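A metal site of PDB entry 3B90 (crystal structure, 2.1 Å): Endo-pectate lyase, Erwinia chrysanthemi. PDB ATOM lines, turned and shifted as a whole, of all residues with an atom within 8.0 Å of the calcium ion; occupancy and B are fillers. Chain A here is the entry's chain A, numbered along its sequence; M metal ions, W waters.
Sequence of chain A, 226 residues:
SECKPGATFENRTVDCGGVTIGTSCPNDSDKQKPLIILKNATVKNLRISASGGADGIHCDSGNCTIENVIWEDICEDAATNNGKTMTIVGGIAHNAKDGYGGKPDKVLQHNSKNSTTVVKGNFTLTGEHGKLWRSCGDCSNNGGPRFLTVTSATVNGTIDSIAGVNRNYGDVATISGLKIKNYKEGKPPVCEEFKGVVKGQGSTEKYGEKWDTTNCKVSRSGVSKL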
ATOM      1  N   CYS A  25       4.078  20.133  -7.788  1.00  0.00           N
ATOM      2  CA  CYS A  25       5.185  20.674  -7.047  1.00  0.00           C
ATOM      3  C   CYS A  25       6.443  20.724  -7.875  1.00  0.00           C
ATOM      4  O   CYS A  25       7.336  19.887  -7.713  1.00  0.00           O
ATOM      5  CB  CYS A  25       5.450  19.896  -5.756  1.00  0.00           C
ATOM      6  SG  CYS A  25       6.905  20.502  -4.830  1.00  0.00           S
ATOM      7  N   ALA A  50       1.762  13.459  -2.421  1.00  0.00           N
ATOM      8  CA  ALA A  50       3.214  13.597  -2.502  1.00  0.00           C
ATOM      9  C   ALA A  50       3.713  14.557  -3.589  1.00  0.00           C
ATOM     10  O   ALA A  50       4.674  15.294  -3.364  1.00  0.00           O
ATOM     11  CB  ALA A  50       3.846  12.225  -2.690  1.00  0.00           C
ATOM     12  N   GLU A  72       2.077  14.067   2.588  1.00  0.00           N
ATOM     13  CA  GLU A  72       2.826  12.926   2.048  1.00  0.00           C
ATOM     14  C   GLU A  72       4.257  13.249   1.612  1.00  0.00           C
ATOM     15  O   GLU A  72       5.113  12.371   1.601  1.00  0.00           O
ATOM     16  CB  GLU A  72       2.024  12.282   0.910  1.00  0.00           C
ATOM     17  CG  GLU A  72       0.932  11.354   1.430  1.00  0.00           C
ATOM     18  CD  GLU A  72      -0.140  11.025   0.408  1.00  0.00           C
ATOM     19  OE1 GLU A  72      -1.287  10.765   0.825  1.00  0.00           O
ATOM     20  OE2 GLU A  72       0.153  11.024  -0.811  1.00  0.00           O
ATOM     21  N   ASP A  73       4.492  14.503   1.231  1.00  0.00           N
ATOM     22  CA  ASP A  73       5.811  14.989   0.832  1.00  0.00           C
ATOM     23  C   ASP A  73       5.703  16.498   0.770  1.00  0.00           C
ATOM     24  O   ASP A  73       5.219  17.050  -0.230  1.00  0.00           O
ATOM     25  CB  ASP A  73       6.238  14.422  -0.543  1.00  0.00           C
ATOM     26  CG  ASP A  73       7.722  14.631  -0.833  1.00  0.00           C
ATOM     27  OD1 ASP A  73       8.387  15.408  -0.115  1.00  0.00           O
ATOM     28  OD2 ASP A  73       8.232  14.012  -1.798  1.00  0.00           O
ATOM     29  N   ILE A  74       6.118  17.161   1.845  1.00  0.00           N
ATOM     30  CA  ILE A  74       6.064  18.633   1.894  1.00  0.00           C
ATOM     31  C   ILE A  74       6.744  19.207   0.652  1.00  0.00           C
ATOM     32  O   ILE A  74       7.845  18.769   0.284  1.00  0.00           O
ATOM     33  CB  ILE A  74       6.804  19.188   3.135  1.00  0.00           C
ATOM     34  CG1 ILE A  74       6.118  18.713   4.419  1.00  0.00           C
ATOM     35  CG2 ILE A  74       6.871  20.717   3.055  1.00  0.00           C
ATOM     36  CD1 ILE A  74       6.787  19.220   5.677  1.00  0.00           C
ATOM     37  N   CYS A  75       6.080  20.133  -0.021  1.00  0.00           N
ATOM     38  CA  CYS A  75       6.653  20.764  -1.203  1.00  0.00           C
ATOM     39  C   CYS A  75       7.504  21.963  -0.796  1.00  0.00           C
ATOM     40  O   CYS A  75       8.712  21.824  -0.598  1.00  0.00           O
ATOM     41  CB  CYS A  75       5.557  21.178  -2.193  1.00  0.00           C
ATOM     42  SG  CYS A  75       6.170  22.028  -3.691  1.00  0.00           S
ATOM     43  N   GLU A  76       6.894  23.131  -0.640  1.00  0.00           N
ATOM     44  CA  GLU A  76       7.652  24.329  -0.229  1.00  0.00           C
ATOM     45  C   GLU A  76       7.769  24.379   1.295  1.00  0.00           C
ATOM     46  O   GLU A  76       8.854  24.562   1.859  1.00  0.00           O
ATOM     47  CB  GLU A  76       6.976  25.597  -0.760  1.00  0.00           C
ATOM     48  CG  GLU A  76       7.883  26.822  -0.731  1.00  0.00           C
ATOM     49  CD  GLU A  76       7.370  27.963  -1.600  1.00  0.00           C
ATOM     50  OE1 GLU A  76       7.545  29.145  -1.222  1.00  0.00           O
ATOM     51  OE2 GLU A  76       6.794  27.671  -2.675  1.00  0.00           O
ATOM     52  N   ASP A  77       6.620  24.265   1.941  1.00  0.00           N
ATOM     53  CA  ASP A  77       6.498  24.239   3.407  1.00  0.00           C
ATOM     54  C   ASP A  77       5.111  23.690   3.707  1.00  0.00           C
ATOM     55  O   ASP A  77       4.253  23.677   2.825  1.00  0.00           O
ATOM     56  CB  ASP A  77       6.745  25.628   4.027  1.00  0.00           C
ATOM     57  CG  ASP A  77       6.081  26.752   3.268  1.00  0.00           C
ATOM     58  OD1 ASP A  77       6.803  27.673   2.818  1.00  0.00           O
ATOM     59  OD2 ASP A  77       4.843  26.740   3.129  1.00  0.00           O
ATOM     60  N   HIS A  94       5.417  14.415   6.330  1.00  0.00           N
ATOM     61  CA  HIS A  94       6.539  13.705   5.735  1.00  0.00           C
ATOM     62  C   HIS A  94       7.283  14.550   4.700  1.00  0.00           C
ATOM     63  O   HIS A  94       6.694  15.368   3.997  1.00  0.00           O
ATOM     64  CB  HIS A  94       6.039  12.417   5.062  1.00  0.00           C
ATOM     65  CG  HIS A  94       7.122  11.619   4.388  1.00  0.00           C
ATOM     66  ND1 HIS A  94       7.745  10.561   5.011  1.00  0.00           N
ATOM     67  CD2 HIS A  94       7.674  11.723   3.159  1.00  0.00           C
ATOM     68  CE1 HIS A  94       8.640  10.037   4.182  1.00  0.00           C
ATOM     69  NE2 HIS A  94       8.617  10.730   3.057  1.00  0.00           N
ATOM     70  N   ASN A  95       8.584  14.315   4.598  1.00  0.00           N
ATOM     71  CA  ASN A  95       9.446  15.007   3.649  1.00  0.00           C
ATOM     72  C   ASN A  95      10.641  14.067   3.427  1.00  0.00           C
ATOM     73  O   ASN A  95      10.915  13.198   4.260  1.00  0.00           O
ATOM     74  CB  ASN A  95       9.900  16.347   4.214  1.00  0.00           C
ATOM     75  CG  ASN A  95      10.242  17.366   3.127  1.00  0.00           C
ATOM     76  OD1 ASN A  95      10.188  17.055   1.931  1.00  0.00           O
ATOM     77  ND2 ASN A  95      10.590  18.582   3.543  1.00  0.00           N
ATOM     78  N   ALA A  96      11.343  14.219   2.304  1.00  0.00           N
ATOM     79  CA  ALA A  96      12.470  13.330   2.042  1.00  0.00           C
ATOM     80  C   ALA A  96      13.551  13.890   1.125  1.00  0.00           C
ATOM     81  O   ALA A  96      13.305  14.768   0.304  1.00  0.00           O
ATOM     82  CB  ALA A  96      11.962  12.007   1.488  1.00  0.00           C
ATOM     83  N   LYS A  97      14.765  13.368   1.295  1.00  0.00           N
ATOM     84  CA  LYS A  97      15.908  13.721   0.461  1.00  0.00           C
ATOM     85  C   LYS A  97      15.528  13.100  -0.881  1.00  0.00           C
ATOM     86  O   LYS A  97      15.084  11.952  -0.912  1.00  0.00           O
ATOM     87  CB  LYS A  97      17.176  13.060   1.007  1.00  0.00           C
ATOM     88  CG  LYS A  97      17.058  11.542   1.135  1.00  0.00           C
ATOM     89  CD  LYS A  97      18.230  10.903   1.866  1.00  0.00           C
ATOM     90  CE  LYS A  97      18.028   9.400   2.000  1.00  0.00           C
ATOM     91  NZ  LYS A  97      18.990   8.799   2.973  1.00  0.00           N
ATOM     92  N   ASP A  98      15.677  13.842  -1.967  1.00  0.00           N
ATOM     93  CA  ASP A  98      15.307  13.321  -3.293  1.00  0.00           C
ATOM     94  C   ASP A  98      13.792  13.287  -3.525  1.00  0.00           C
ATOM     95  O   ASP A  98      13.318  12.621  -4.438  1.00  0.00           O
ATOM     96  CB  ASP A  98      15.899  11.937  -3.538  1.00  0.00           C
ATOM     97  CG  ASP A  98      17.169  11.981  -4.371  1.00  0.00           C
ATOM     98  OD1 ASP A  98      17.088  11.618  -5.564  1.00  0.00           O
ATOM     99  OD2 ASP A  98      18.222  12.374  -3.827  1.00  0.00           O
ATOM    100  N   GLY A  99      13.043  13.993  -2.683  1.00  0.00           N
ATOM    101  CA  GLY A  99      11.599  14.043  -2.838  1.00  0.00           C
ATOM    102  C   GLY A  99      11.187  15.213  -3.710  1.00  0.00           C
ATOM    103  O   GLY A  99      11.977  15.702  -4.515  1.00  0.00           O
ATOM    104  N   TYR A 100       9.932  15.637  -3.557  1.00  0.00           N
ATOM    105  CA  TYR A 100       9.393  16.762  -4.330  1.00  0.00           C
ATOM    106  C   TYR A 100       9.671  18.077  -3.625  1.00  0.00           C
ATOM    107  O   TYR A 100       9.512  18.180  -2.403  1.00  0.00           O
ATOM    108  CB  TYR A 100       7.893  16.573  -4.574  1.00  0.00           C
ATOM    109  CG  TYR A 100       7.613  15.594  -5.697  1.00  0.00           C
ATOM    110  CD1 TYR A 100       7.165  14.301  -5.420  1.00  0.00           C
ATOM    111  CD2 TYR A 100       7.888  15.931  -7.019  1.00  0.00           C
ATOM    112  CE1 TYR A 100       7.007  13.367  -6.441  1.00  0.00           C
ATOM    113  CE2 TYR A 100       7.750  14.999  -8.037  1.00  0.00           C
ATOM    114  CZ  TYR A 100       7.308  13.721  -7.744  1.00  0.00           C
ATOM    115  OH  TYR A 100       7.218  12.793  -8.753  1.00  0.00           O
ATOM    116  N   GLY A 101      10.117  19.073  -4.383  1.00  0.00           N
ATOM    117  CA  GLY A 101      10.419  20.373  -3.803  1.00  0.00           C
ATOM    118  C   GLY A 101      11.876  20.546  -3.423  1.00  0.00           C
ATOM    119  O   GLY A 101      12.234  21.512  -2.732  1.00  0.00           O
ATOM    120  N   GLY A 102      12.718  19.598  -3.831  1.00  0.00           N
ATOM    121  CA  GLY A 102      14.150  19.662  -3.549  1.00  0.00           C
ATOM    122  C   GLY A 102      14.585  19.217  -2.162  1.00  0.00           C
ATOM    123  O   GLY A 102      13.958  18.361  -1.537  1.00  0.00           O
ATOM    124  N   LYS A 103      15.702  19.783  -1.707  1.00  0.00           N
ATOM    125  CA  LYS A 103      16.248  19.481  -0.379  1.00  0.00           C
ATOM    126  C   LYS A 103      15.272  19.988   0.680  1.00  0.00           C
ATOM    127  O   LYS A 103      14.807  21.129   0.610  1.00  0.00           O
ATOM    128  CB  LYS A 103      17.601  20.182  -0.219  1.00  0.00           C
ATOM    129  CG  LYS A 103      18.191  20.154   1.204  1.00  0.00           C
ATOM    130  CD  LYS A 103      19.559  20.827   1.237  1.00  0.00           C
ATOM    131  CE  LYS A 103      19.995  21.198   2.661  1.00  0.00           C
ATOM    132  NZ  LYS A 103      20.138  20.015   3.563  1.00  0.00           N
ATOM    133  N   PRO A 104      14.901  19.114   1.640  1.00  0.00           N
ATOM    134  CA  PRO A 104      13.973  19.419   2.743  1.00  0.00           C
ATOM    135  C   PRO A 104      14.317  20.718   3.482  1.00  0.00           C
ATOM    136  O   PRO A 104      15.470  20.952   3.821  1.00  0.00           O
ATOM    137  CB  PRO A 104      14.127  18.202   3.654  1.00  0.00           C
ATOM    138  CG  PRO A 104      14.313  17.097   2.667  1.00  0.00           C
ATOM    139  CD  PRO A 104      15.302  17.691   1.676  1.00  0.00           C
ATOM    140  N   ASP A 105      13.307  21.538   3.745  1.00  0.00           N
ATOM    141  CA  ASP A 105      13.523  22.818   4.410  1.00  0.00           C
ATOM    142  C   ASP A 105      12.595  23.004   5.621  1.00  0.00           C
ATOM    143  O   ASP A 105      12.518  22.137   6.476  1.00  0.00           O
ATOM    144  CB  ASP A 105      13.342  23.954   3.401  1.00  0.00           C
ATOM    145  CG  ASP A 105      14.317  25.109   3.593  1.00  0.00           C
ATOM    146  OD1 ASP A 105      15.246  25.000   4.416  1.00  0.00           O
ATOM    147  OD2 ASP A 105      14.159  26.131   2.897  1.00  0.00           O
ATOM    148  N   GLU A 128      12.997  12.869   5.961  1.00  0.00           N
ATOM    149  CA  GLU A 128      14.088  13.814   6.167  1.00  0.00           C
ATOM    150  C   GLU A 128      13.555  15.241   6.179  1.00  0.00           C
ATOM    151  O   GLU A 128      12.854  15.643   5.261  1.00  0.00           O
ATOM    152  CB  GLU A 128      15.138  13.659   5.057  1.00  0.00           C
ATOM    153  CG  GLU A 128      15.921  12.351   5.076  1.00  0.00           C
ATOM    154  CD  GLU A 128      15.134  11.177   4.530  1.00  0.00           C
ATOM    155  OE1 GLU A 128      14.734  11.216   3.350  1.00  0.00           O
ATOM    156  OE2 GLU A 128      14.911  10.205   5.279  1.00  0.00           O
ATOM    157  N   HIS A 129      13.930  16.014   7.203  1.00  0.00           N
ATOM    158  CA  HIS A 129      13.461  17.405   7.327  1.00  0.00           C
ATOM    159  C   HIS A 129      14.526  18.469   7.565  1.00  0.00           C
ATOM    160  O   HIS A 129      15.643  18.177   7.998  1.00  0.00           O
ATOM    161  CB  HIS A 129      12.413  17.531   8.438  1.00  0.00           C
ATOM    162  CG  HIS A 129      11.073  16.956   8.093  1.00  0.00           C
ATOM    163  ND1 HIS A 129      10.047  17.722   7.576  1.00  0.00           N
ATOM    164  CD2 HIS A 129      10.572  15.707   8.253  1.00  0.00           C
ATOM    165  CE1 HIS A 129       8.969  16.971   7.437  1.00  0.00           C
ATOM    166  NE2 HIS A 129       9.257  15.743   7.841  1.00  0.00           N
HETATM  167 CA    CA M   1       9.721  17.523  -0.188  1.00  0.00          CA
HETATM  168  O   HOH W   1      11.795  16.819  -0.580  1.00  0.00           O
HETATM  169  O   HOH W   2      10.546  19.877   0.309  1.00  0.00           O
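The backbone carbonyl oxygen of Asn 95 is in hydrogen-bond range of the backbone NH of Glu 128 (2.7 Å).
N of Ile 74 sits at hydrogen-bond distance from O of His 94, at 2.9 Å.
The side-chain sulfur of Cys 75 forms a disulfide with the side-chain sulfur of Cys 25 (2.0 Å).
Four residues have an atom within 4 Å of the calcium ion: Asp 73, Ile 74, Asn 95 and Tyr 100.
The nearest printed residue that does not touch the calcium ion is Cys 75 (4.4 Å).
The calcium ion is bound by the side-chain amide oxygen of Asn 95 (2.2 Å), water W1 (2.2 Å), the backbone carbonyl oxygen of Ile 74 (2.3 Å), the backbone carbonyl oxygen of Tyr 100 (2.3 Å), the side-chain carboxylate of Asp 73 (2.5 Å) and water W2 (2.5 Å).
The calcium ion has six donor atoms within binding distance.
Water W2 bridges the backbone carbonyl oxygen of Cys 75 and the side-chain amide nitrogen of Asn 95.
Water W1 lies within hydrogen-bond range of the backbone carbonyl oxygen (O) of Ala 96 (2.7 Å) and the backbone carbonyl oxygen (O) of Gly 102 (2.8 Å).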
